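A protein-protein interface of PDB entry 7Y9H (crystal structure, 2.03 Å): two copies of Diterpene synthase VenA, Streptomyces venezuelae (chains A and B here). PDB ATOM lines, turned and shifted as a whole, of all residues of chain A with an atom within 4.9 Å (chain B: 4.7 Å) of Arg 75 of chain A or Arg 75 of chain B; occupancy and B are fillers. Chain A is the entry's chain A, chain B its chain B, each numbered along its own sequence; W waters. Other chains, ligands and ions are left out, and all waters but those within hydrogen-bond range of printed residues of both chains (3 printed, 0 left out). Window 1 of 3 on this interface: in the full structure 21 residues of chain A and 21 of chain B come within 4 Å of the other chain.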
ATOM      1  N   GLU A  47       2.120 -14.952  -9.708  1.00  0.00           N
ATOM      2  CA  GLU A  47       1.394 -13.955  -8.883  1.00  0.00           C
ATOM      3  C   GLU A  47       1.912 -12.561  -9.229  1.00  0.00           C
ATOM      4  O   GLU A  47       1.061 -11.652  -9.496  1.00  0.00           O
ATOM      5  CB  GLU A  47       1.575 -14.273  -7.398  1.00  0.00           C
ATOM      6  CG  GLU A  47       0.938 -13.238  -6.487  1.00  0.00           C
ATOM      7  CD  GLU A  47       1.211 -13.472  -5.009  1.00  0.00           C
ATOM      8  OE1 GLU A  47       2.068 -14.349  -4.707  1.00  0.00           O
ATOM      9  OE2 GLU A  47       0.587 -12.784  -4.151  1.00  0.00           O
ATOM     10  N   ILE A  48       3.244 -12.393  -9.208  1.00  0.00           N
ATOM     11  CA  ILE A  48       3.889 -11.087  -9.529  1.00  0.00           C
ATOM     12  C   ILE A  48       3.480 -10.642 -10.935  1.00  0.00           C
ATOM     13  O   ILE A  48       3.136  -9.468 -11.119  1.00  0.00           O
ATOM     14  CB  ILE A  48       5.430 -11.191  -9.393  1.00  0.00           C
ATOM     15  CG1 ILE A  48       5.863 -11.573  -7.985  1.00  0.00           C
ATOM     16  CG2 ILE A  48       6.080  -9.901  -9.870  1.00  0.00           C
ATOM     17  CD1 ILE A  48       5.053 -10.877  -6.910  1.00  0.00           C
ATOM     18  N   PHE A  71      -5.826  -3.798  -3.216  1.00  0.00           N
ATOM     19  CA  PHE A  71      -6.290  -4.961  -4.016  1.00  0.00           C
ATOM     20  C   PHE A  71      -5.145  -5.958  -4.262  1.00  0.00           C
ATOM     21  O   PHE A  71      -5.309  -7.173  -4.097  1.00  0.00           O
ATOM     22  CB  PHE A  71      -6.894  -4.502  -5.333  1.00  0.00           C
ATOM     23  CG  PHE A  71      -7.295  -5.681  -6.183  1.00  0.00           C
ATOM     24  CD1 PHE A  71      -8.516  -6.314  -5.976  1.00  0.00           C
ATOM     25  CD2 PHE A  71      -6.423  -6.197  -7.131  1.00  0.00           C
ATOM     26  CE1 PHE A  71      -8.870  -7.417  -6.732  1.00  0.00           C
ATOM     27  CE2 PHE A  71      -6.792  -7.284  -7.909  1.00  0.00           C
ATOM     28  CZ  PHE A  71      -8.013  -7.887  -7.707  1.00  0.00           C
ATOM     29  N   LEU A  72      -3.969  -5.463  -4.644  1.00  0.00           N
ATOM     30  CA  LEU A  72      -2.801  -6.338  -4.884  1.00  0.00           C
ATOM     31  C   LEU A  72      -2.359  -7.057  -3.621  1.00  0.00           C
ATOM     32  O   LEU A  72      -1.955  -8.219  -3.752  1.00  0.00           O
ATOM     33  CB  LEU A  72      -1.660  -5.518  -5.468  1.00  0.00           C
ATOM     34  CG  LEU A  72      -1.949  -4.959  -6.851  1.00  0.00           C
ATOM     35  CD1 LEU A  72      -0.728  -4.228  -7.353  1.00  0.00           C
ATOM     36  CD2 LEU A  72      -2.365  -6.057  -7.825  1.00  0.00           C
ATOM     37  N   ARG A  73      -2.452  -6.418  -2.445  1.00  0.00           N
ATOM     38  CA  ARG A  73      -2.097  -7.070  -1.172  1.00  0.00           C
ATOM     39  C   ARG A  73      -2.989  -8.289  -0.885  1.00  0.00           C
ATOM     40  O   ARG A  73      -2.605  -9.134   0.015  1.00  0.00           O
ATOM     41  CB  ARG A  73      -2.117  -6.040  -0.044  1.00  0.00           C
ATOM     42  CG  ARG A  73      -0.839  -5.236   0.017  1.00  0.00           C
ATOM     43  CD  ARG A  73      -0.713  -4.443   1.274  1.00  0.00           C
ATOM     44  NE  ARG A  73      -1.865  -3.591   1.551  1.00  0.00           N
ATOM     45  CZ  ARG A  73      -2.051  -2.343   1.105  1.00  0.00           C
ATOM     46  NH1 ARG A  73      -1.233  -1.770   0.253  1.00  0.00           N
ATOM     47  NH2 ARG A  73      -3.127  -1.679   1.466  1.00  0.00           N
ATOM     48  N   GLN A  74      -4.108  -8.465  -1.596  1.00  0.00           N
ATOM     49  CA  GLN A  74      -5.001  -9.625  -1.334  1.00  0.00           C
ATOM     50  C   GLN A  74      -4.400 -10.901  -1.909  1.00  0.00           C
ATOM     51  O   GLN A  74      -4.905 -11.995  -1.576  1.00  0.00           O
ATOM     52  CB  GLN A  74      -6.385  -9.373  -1.916  1.00  0.00           C
ATOM     53  CG  GLN A  74      -7.006  -8.117  -1.344  1.00  0.00           C
ATOM     54  CD  GLN A  74      -8.390  -7.859  -1.862  1.00  0.00           C
ATOM     55  OE1 GLN A  74      -8.819  -8.463  -2.842  1.00  0.00           O
ATOM     56  NE2 GLN A  74      -9.106  -7.021  -1.133  1.00  0.00           N
ATOM     57  N   ARG A  75      -3.324 -10.787  -2.682  1.00  0.00           N
ATOM     58  CA  ARG A  75      -2.658 -11.967  -3.312  1.00  0.00           C
ATOM     59  C   ARG A  75      -3.633 -12.755  -4.207  1.00  0.00           C
ATOM     60  O   ARG A  75      -3.433 -13.964  -4.377  1.00  0.00           O
ATOM     61  CB  ARG A  75      -2.059 -12.843  -2.218  1.00  0.00           C
ATOM     62  CG  ARG A  75      -0.981 -12.125  -1.416  1.00  0.00           C
ATOM     63  CD  ARG A  75      -0.148 -13.113  -0.636  1.00  0.00           C
ATOM     64  NE  ARG A  75       0.655 -13.895  -1.549  1.00  0.00           N
ATOM     65  CZ  ARG A  75       1.358 -14.969  -1.219  1.00  0.00           C
ATOM     66  NH1 ARG A  75       1.309 -15.466   0.013  1.00  0.00           N
ATOM     67  NH2 ARG A  75       2.082 -15.561  -2.146  1.00  0.00           N
ATOM     68  N   ASN A  76      -4.593 -12.101  -4.858  1.00  0.00           N
ATOM     69  CA  ASN A  76      -5.558 -12.815  -5.737  1.00  0.00           C
ATOM     70  C   ASN A  76      -4.774 -13.503  -6.876  1.00  0.00           C
ATOM     71  O   ASN A  76      -5.289 -14.469  -7.451  1.00  0.00           O
ATOM     72  CB  ASN A  76      -6.666 -11.882  -6.240  1.00  0.00           C
ATOM     73  CG  ASN A  76      -7.519 -11.349  -5.102  1.00  0.00           C
ATOM     74  OD1 ASN A  76      -8.009 -12.121  -4.269  1.00  0.00           O
ATOM     75  ND2 ASN A  76      -7.655 -10.035  -5.039  1.00  0.00           N
ATOM     76  N   GLY A  77      -3.589 -13.000  -7.215  1.00  0.00           N
ATOM     77  CA  GLY A  77      -2.722 -13.548  -8.263  1.00  0.00           C
ATOM     78  C   GLY A  77      -2.197 -14.948  -7.976  1.00  0.00           C
ATOM     79  O   GLY A  77      -1.733 -15.587  -8.941  1.00  0.00           O
ATOM     80  N   ILE A  78      -2.197 -15.405  -6.720  1.00  0.00           N
ATOM     81  CA  ILE A  78      -1.786 -16.789  -6.378  1.00  0.00           C
ATOM     82  C   ILE A  78      -2.979 -17.763  -6.454  1.00  0.00           C
ATOM     83  O   ILE A  78      -2.710 -18.987  -6.406  1.00  0.00           O
ATOM     84  CB  ILE A  78      -1.048 -16.856  -5.033  1.00  0.00           C
ATOM     85  CG1 ILE A  78      -0.128 -18.074  -5.037  1.00  0.00           C
ATOM     86  CG2 ILE A  78      -1.980 -16.853  -3.820  1.00  0.00           C
ATOM     87  CD1 ILE A  78       1.305 -17.781  -4.826  1.00  0.00           C
ATOM     88  N   TYR A  79      -4.228 -17.283  -6.575  1.00  0.00           N
ATOM     89  CA  TYR A  79      -5.398 -18.180  -6.749  1.00  0.00           C
ATOM     90  C   TYR A  79      -5.110 -19.113  -7.939  1.00  0.00           C
ATOM     91  O   TYR A  79      -5.164 -20.358  -7.773  1.00  0.00           O
ATOM     92  CB  TYR A  79      -6.732 -17.436  -6.888  1.00  0.00           C
ATOM     93  CG  TYR A  79      -7.836 -18.352  -7.376  1.00  0.00           C
ATOM     94  CD1 TYR A  79      -7.983 -18.588  -8.747  1.00  0.00           C
ATOM     95  CD2 TYR A  79      -8.643 -19.093  -6.511  1.00  0.00           C
ATOM     96  CE1 TYR A  79      -8.943 -19.456  -9.246  1.00  0.00           C
ATOM     97  CE2 TYR A  79      -9.634 -19.954  -6.995  1.00  0.00           C
ATOM     98  CZ  TYR A  79      -9.757 -20.164  -8.369  1.00  0.00           C
ATOM     99  OH  TYR A  79     -10.665 -21.038  -8.944  1.00  0.00           O
ATOM    100  N   PHE A 329      -6.182 -21.177  -0.850  1.00  0.00           N
ATOM    101  CA  PHE A 329      -6.211 -19.754  -1.243  1.00  0.00           C
ATOM    102  C   PHE A 329      -7.077 -18.934  -0.269  1.00  0.00           C
ATOM    103  O   PHE A 329      -6.641 -17.864   0.184  1.00  0.00           O
ATOM    104  CB  PHE A 329      -6.704 -19.545  -2.683  1.00  0.00           C
ATOM    105  CG  PHE A 329      -6.853 -18.076  -2.971  1.00  0.00           C
ATOM    106  CD1 PHE A 329      -5.720 -17.272  -3.094  1.00  0.00           C
ATOM    107  CD2 PHE A 329      -8.100 -17.466  -2.935  1.00  0.00           C
ATOM    108  CE1 PHE A 329      -5.839 -15.892  -3.252  1.00  0.00           C
ATOM    109  CE2 PHE A 329      -8.219 -16.086  -3.077  1.00  0.00           C
ATOM    110  CZ  PHE A 329      -7.093 -15.309  -3.267  1.00  0.00           C
ATOM    111  N   LEU A 332      -5.471 -18.076   2.975  1.00  0.00           N
ATOM    112  CA  LEU A 332      -4.273 -17.205   2.903  1.00  0.00           C
ATOM    113  C   LEU A 332      -4.616 -15.754   2.583  1.00  0.00           C
ATOM    114  O   LEU A 332      -3.806 -14.873   2.959  1.00  0.00           O
ATOM    115  CB  LEU A 332      -3.192 -17.825   2.007  1.00  0.00           C
ATOM    116  CG  LEU A 332      -3.075 -17.561   0.512  1.00  0.00           C
ATOM    117  CD1 LEU A 332      -2.612 -16.158   0.137  1.00  0.00           C
ATOM    118  CD2 LEU A 332      -2.044 -18.543  -0.057  1.00  0.00           C
ATOM    119  N   THR A 333      -5.726 -15.470   1.908  1.00  0.00           N
ATOM    120  CA  THR A 333      -5.944 -14.135   1.296  1.00  0.00           C
ATOM    121  C   THR A 333      -6.284 -13.096   2.358  1.00  0.00           C
ATOM    122  O   THR A 333      -7.208 -13.278   3.135  1.00  0.00           O
ATOM    123  CB  THR A 333      -6.979 -14.165   0.169  1.00  0.00           C
ATOM    124  OG1 THR A 333      -7.047 -12.818  -0.308  1.00  0.00           O
ATOM    125  CG2 THR A 333      -8.325 -14.699   0.596  1.00  0.00           C
ATOM    126  N   PRO A 334      -5.568 -11.943   2.391  1.00  0.00           N
ATOM    127  CA  PRO A 334      -6.013 -10.773   3.157  1.00  0.00           C
ATOM    128  C   PRO A 334      -7.389 -10.218   2.747  1.00  0.00           C
ATOM    129  O   PRO A 334      -7.928  -9.398   3.471  1.00  0.00           O
ATOM    130  CB  PRO A 334      -4.935  -9.723   2.861  1.00  0.00           C
ATOM    131  CG  PRO A 334      -3.694 -10.560   2.578  1.00  0.00           C
ATOM    132  CD  PRO A 334      -4.251 -11.728   1.768  1.00  0.00           C
ATOM    133  N   GLU B  47       7.604 -19.887   1.753  1.00  0.00           N
ATOM    134  CA  GLU B  47       7.436 -18.540   2.375  1.00  0.00           C
ATOM    135  C   GLU B  47       6.381 -18.636   3.496  1.00  0.00           C
ATOM    136  O   GLU B  47       6.637 -18.164   4.617  1.00  0.00           O
ATOM    137  CB  GLU B  47       7.072 -17.515   1.306  1.00  0.00           C
ATOM    138  CG  GLU B  47       6.706 -16.145   1.855  1.00  0.00           C
ATOM    139  CD  GLU B  47       6.220 -15.167   0.800  1.00  0.00           C
ATOM    140  OE1 GLU B  47       5.955 -15.586  -0.386  1.00  0.00           O
ATOM    141  OE2 GLU B  47       6.103 -13.978   1.162  1.00  0.00           O
ATOM    142  N   ILE B  48       5.223 -19.232   3.197  1.00  0.00           N
ATOM    143  CA  ILE B  48       4.117 -19.411   4.184  1.00  0.00           C
ATOM    144  C   ILE B  48       4.616 -20.266   5.350  1.00  0.00           C
ATOM    145  O   ILE B  48       4.382 -19.881   6.508  1.00  0.00           O
ATOM    146  CB  ILE B  48       2.871 -20.017   3.518  1.00  0.00           C
ATOM    147  CG1 ILE B  48       2.299 -19.057   2.485  1.00  0.00           C
ATOM    148  CG2 ILE B  48       1.837 -20.374   4.568  1.00  0.00           C
ATOM    149  CD1 ILE B  48       1.532 -19.738   1.398  1.00  0.00           C
ATOM    150  N   PHE B  71       6.855  -7.187   9.771  1.00  0.00           N
ATOM    151  CA  PHE B  71       7.992  -8.054   9.390  1.00  0.00           C
ATOM    152  C   PHE B  71       7.559  -9.112   8.369  1.00  0.00           C
ATOM    153  O   PHE B  71       8.239  -9.266   7.342  1.00  0.00           O
ATOM    154  CB  PHE B  71       8.626  -8.672  10.640  1.00  0.00           C
ATOM    155  CG  PHE B  71       9.757  -9.573  10.246  1.00  0.00           C
ATOM    156  CD1 PHE B  71      10.975  -9.027   9.869  1.00  0.00           C
ATOM    157  CD2 PHE B  71       9.566 -10.937  10.149  1.00  0.00           C
ATOM    158  CE1 PHE B  71      11.994  -9.855   9.445  1.00  0.00           C
ATOM    159  CE2 PHE B  71      10.584 -11.759   9.709  1.00  0.00           C
ATOM    160  CZ  PHE B  71      11.790 -11.219   9.374  1.00  0.00           C
ATOM    161  N   LEU B  72       6.474  -9.865   8.634  1.00  0.00           N
ATOM    162  CA  LEU B  72       6.040 -10.940   7.701  1.00  0.00           C
ATOM    163  C   LEU B  72       5.688 -10.332   6.335  1.00  0.00           C
ATOM    164  O   LEU B  72       5.905 -11.031   5.300  1.00  0.00           O
ATOM    165  CB  LEU B  72       4.893 -11.775   8.294  1.00  0.00           C
ATOM    166  CG  LEU B  72       5.217 -12.470   9.610  1.00  0.00           C
ATOM    167  CD1 LEU B  72       3.990 -13.192  10.154  1.00  0.00           C
ATOM    168  CD2 LEU B  72       6.383 -13.431   9.465  1.00  0.00           C
ATOM    169  N   ARG B  73       5.236  -9.076   6.283  1.00  0.00           N
ATOM    170  CA  ARG B  73       4.819  -8.439   5.001  1.00  0.00           C
ATOM    171  C   ARG B  73       6.053  -8.184   4.129  1.00  0.00           C
ATOM    172  O   ARG B  73       5.869  -7.994   2.912  1.00  0.00           O
ATOM    173  CB  ARG B  73       3.982  -7.173   5.225  1.00  0.00           C
ATOM    174  CG  ARG B  73       2.545  -7.465   5.650  1.00  0.00           C
ATOM    175  CD  ARG B  73       1.647  -6.262   5.483  1.00  0.00           C
ATOM    176  NE  ARG B  73       2.036  -5.124   6.309  1.00  0.00           N
ATOM    177  CZ  ARG B  73       1.711  -4.953   7.583  1.00  0.00           C
ATOM    178  NH1 ARG B  73       1.040  -5.879   8.240  1.00  0.00           N
ATOM    179  NH2 ARG B  73       2.116  -3.871   8.222  1.00  0.00           N
ATOM    180  N   GLN B  74       7.270  -8.221   4.690  1.00  0.00           N
ATOM    181  CA  GLN B  74       8.502  -7.995   3.911  1.00  0.00           C
ATOM    182  C   GLN B  74       8.769  -9.208   3.024  1.00  0.00           C
ATOM    183  O   GLN B  74       9.543  -9.069   2.099  1.00  0.00           O
ATOM    184  CB  GLN B  74       9.685  -7.693   4.822  1.00  0.00           C
ATOM    185  CG  GLN B  74       9.497  -6.378   5.550  1.00  0.00           C
ATOM    186  CD  GLN B  74      10.615  -6.086   6.508  1.00  0.00           C
ATOM    187  OE1 GLN B  74      11.542  -6.884   6.675  1.00  0.00           O
ATOM    188  NE2 GLN B  74      10.548  -4.907   7.108  1.00  0.00           N
ATOM    189  N   ARG B  75       8.111 -10.339   3.268  1.00  0.00           N
ATOM    190  CA  ARG B  75       8.252 -11.535   2.410  1.00  0.00           C
ATOM    191  C   ARG B  75       9.706 -12.050   2.467  1.00  0.00           C
ATOM    192  O   ARG B  75      10.200 -12.648   1.489  1.00  0.00           O
ATOM    193  CB  ARG B  75       7.816 -11.186   0.989  1.00  0.00           C
ATOM    194  CG  ARG B  75       6.406 -10.629   0.847  1.00  0.00           C
ATOM    195  CD  ARG B  75       5.928 -10.693  -0.599  1.00  0.00           C
ATOM    196  NE  ARG B  75       5.885 -12.094  -1.003  1.00  0.00           N
ATOM    197  CZ  ARG B  75       5.658 -12.517  -2.219  1.00  0.00           C
ATOM    198  NH1 ARG B  75       5.472 -11.658  -3.218  1.00  0.00           N
ATOM    199  NH2 ARG B  75       5.629 -13.820  -2.437  1.00  0.00           N
ATOM    200  N   ASN B  76      10.369 -11.900   3.601  1.00  0.00           N
ATOM    201  CA  ASN B  76      11.757 -12.376   3.796  1.00  0.00           C
ATOM    202  C   ASN B  76      11.761 -13.892   3.660  1.00  0.00           C
ATOM    203  O   ASN B  76      12.808 -14.454   3.283  1.00  0.00           O
ATOM    204  CB  ASN B  76      12.316 -11.901   5.131  1.00  0.00           C
ATOM    205  CG  ASN B  76      12.506 -10.400   5.142  1.00  0.00           C
ATOM    206  OD1 ASN B  76      13.077  -9.844   4.205  1.00  0.00           O
ATOM    207  ND2 ASN B  76      11.957  -9.752   6.143  1.00  0.00           N
ATOM    208  N   GLY B  77      10.611 -14.514   3.927  1.00  0.00           N
ATOM    209  CA  GLY B  77      10.453 -15.969   3.811  1.00  0.00           C
ATOM    210  C   GLY B  77      10.689 -16.492   2.405  1.00  0.00           C
ATOM    211  O   GLY B  77      10.864 -17.724   2.295  1.00  0.00           O
ATOM    212  N   ILE B  78      10.622 -15.656   1.358  1.00  0.00           N
ATOM    213  CA  ILE B  78      10.827 -16.136  -0.041  1.00  0.00           C
ATOM    214  C   ILE B  78      12.294 -15.898  -0.500  1.00  0.00           C
ATOM    215  O   ILE B  78      12.630 -16.359  -1.579  1.00  0.00           O
ATOM    216  CB  ILE B  78       9.810 -15.548  -1.031  1.00  0.00           C
ATOM    217  CG1 ILE B  78       9.586 -16.533  -2.183  1.00  0.00           C
ATOM    218  CG2 ILE B  78      10.251 -14.172  -1.544  1.00  0.00           C
ATOM    219  CD1 ILE B  78       8.445 -16.172  -3.078  1.00  0.00           C
ATOM    220  N   TYR B  79      13.147 -15.289   0.326  1.00  0.00           N
ATOM    221  CA  TYR B  79      14.593 -15.111   0.016  1.00  0.00           C
ATOM    222  C   TYR B  79      15.264 -16.484  -0.184  1.00  0.00           C
ATOM    223  O   TYR B  79      15.947 -16.717  -1.205  1.00  0.00           O
ATOM    224  CB  TYR B  79      15.298 -14.274   1.090  1.00  0.00           C
ATOM    225  CG  TYR B  79      16.795 -14.216   0.908  1.00  0.00           C
ATOM    226  CD1 TYR B  79      17.372 -13.343   0.004  1.00  0.00           C
ATOM    227  CD2 TYR B  79      17.627 -15.096   1.575  1.00  0.00           C
ATOM    228  CE1 TYR B  79      18.743 -13.310  -0.191  1.00  0.00           C
ATOM    229  CE2 TYR B  79      19.004 -15.081   1.387  1.00  0.00           C
ATOM    230  CZ  TYR B  79      19.557 -14.185   0.500  1.00  0.00           C
ATOM    231  OH  TYR B  79      20.905 -14.219   0.305  1.00  0.00           O
ATOM    232  N   PHE B 329      14.934 -11.101  -5.424  1.00  0.00           N
ATOM    233  CA  PHE B 329      14.335 -10.910  -4.091  1.00  0.00           C
ATOM    234  C   PHE B 329      14.283  -9.412  -3.734  1.00  0.00           C
ATOM    235  O   PHE B 329      13.288  -8.919  -3.098  1.00  0.00           O
ATOM    236  CB  PHE B 329      15.074 -11.683  -2.999  1.00  0.00           C
ATOM    237  CG  PHE B 329      14.535 -11.310  -1.652  1.00  0.00           C
ATOM    238  CD1 PHE B 329      13.280 -11.767  -1.262  1.00  0.00           C
ATOM    239  CD2 PHE B 329      15.248 -10.487  -0.800  1.00  0.00           C
ATOM    240  CE1 PHE B 329      12.738 -11.385  -0.046  1.00  0.00           C
ATOM    241  CE2 PHE B 329      14.697 -10.091   0.413  1.00  0.00           C
ATOM    242  CZ  PHE B 329      13.454 -10.546   0.790  1.00  0.00           C
ATOM    243  N   LEU B 332      11.554  -7.451  -5.025  1.00  0.00           N
ATOM    244  CA  LEU B 332      10.248  -8.053  -4.609  1.00  0.00           C
ATOM    245  C   LEU B 332       9.821  -7.480  -3.237  1.00  0.00           C
ATOM    246  O   LEU B 332       8.597  -7.271  -2.977  1.00  0.00           O
ATOM    247  CB  LEU B 332      10.476  -9.577  -4.624  1.00  0.00           C
ATOM    248  CG  LEU B 332       9.399 -10.530  -4.103  1.00  0.00           C
ATOM    249  CD1 LEU B 332       9.346 -10.543  -2.578  1.00  0.00           C
ATOM    250  CD2 LEU B 332       8.050 -10.195  -4.667  1.00  0.00           C
ATOM    251  N   PRO B 334       8.836  -5.592   0.158  1.00  0.00           N
ATOM    252  CA  PRO B 334       8.425  -4.376   0.848  1.00  0.00           C
ATOM    253  C   PRO B 334       9.443  -3.864   1.870  1.00  0.00           C
ATOM    254  O   PRO B 334       9.289  -2.723   2.323  1.00  0.00           O
ATOM    255  CB  PRO B 334       7.138  -4.798   1.565  1.00  0.00           C
ATOM    256  CG  PRO B 334       6.580  -5.840   0.644  1.00  0.00           C
ATOM    257  CD  PRO B 334       7.812  -6.633   0.255  1.00  0.00           C
HETATM  258  O   HOH W   1       3.493 -13.147   0.097  1.00  0.00           O
HETATM  259  O   HOH W   2       3.858 -17.209  -0.589  1.00  0.00           O
HETATM  260  O   HOH W   3       4.623 -13.985  -5.317  1.00  0.00           O
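NH2 of Arg 75 of chain B lies within salt-bridge range of OE1 of Glu 47 of chain B, 2.7 Å away. OE2 of Glu 47 of chain A is in salt-bridge range of NE of Arg 75 of chain A (2.8 Å).
Arg 75 of chain B touches Ile 48 of chain A (NH1 to CD1, 3.8 Å). CD2 of Leu 332 of chain B touches CD1 of Ile 48 of chain A, 3.8 Å away. Arg 75 of chain A touches Arg 75 of chain B (NH2 to NH2, 3.96 Å).
Arg 75 of chain A touches just one residue of chain B: Arg 75 (3.96 Å). Of the printed residues of chain A, Arg 75 of chain B touches Ile 48 and Arg 75. Of the printed residues of chain A, Leu 332 of chain B touches Ile 48 (3.8 Å). Of the printed residues of chain B, Ile 48 of chain A touches Arg 75 (3.8 Å) and Leu 332 (3.8 Å). Phe 71 of chain A touches none of the printed residues of chain B. Pro 334 of chain B touches none of the printed residues of chain A. The nearest residue of chain B that does not touch Arg 75 of chain A is Glu 47 of chain B (4.3 Å). The nearest residue of chain A that does not touch Arg 75 of chain B is Glu 47 of chain A (4.3 Å).
Of the 15 printed residues of chain A, 2 touch a printed residue of chain B. Hydrophobic or aromatic side chains of chain A within 4 Å of the printed part of chain B: Ile 48. Along chain A the printed residues that touch a printed residue of chain B span positions 48 to 75. Hydrophobic or aromatic side chains of chain B that line the printed part of chain A: Leu 332.
Ile 48 of chain A touches Arg 75 of chain B, but with the chains exchanged Arg 75 of chain A does not touch Ile 48 of chain B (4.5 Å). Ile 48 of chain A touches Leu 332 of chain B, but with the chains exchanged Leu 332 of chain A does not touch Ile 48 of chain B (4.04 Å). Arg 75 of chain B touches its own counterpart, Arg 75 of chain A. Of the 3 pairs that touch across the chains among the printed residues, 1 has its exchanged pair printed and touching as well.
Water W3 lies within hydrogen-bond range of the side-chain carboxylate (OE1) of Glu 47 of chain A (2.7 Å) and the guanidinium group (NH2) of Arg 75 of chain B (3.1 Å). Water W2 bridges the side-chain carboxylate of Glu 47 of chain B (2.7 Å) and the guanidinium group of Arg 75 of chain A (2.9 Å). Water W1 lies within hydrogen-bond range of the guanidinium group (NE) of Arg 75 of chain B (2.8 Å), the side-chain carboxylate (OE2) of Glu 47 of chain B (2.9 Å) and the guanidinium group (NH1) of Arg 75 of chain A (3.2 Å).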
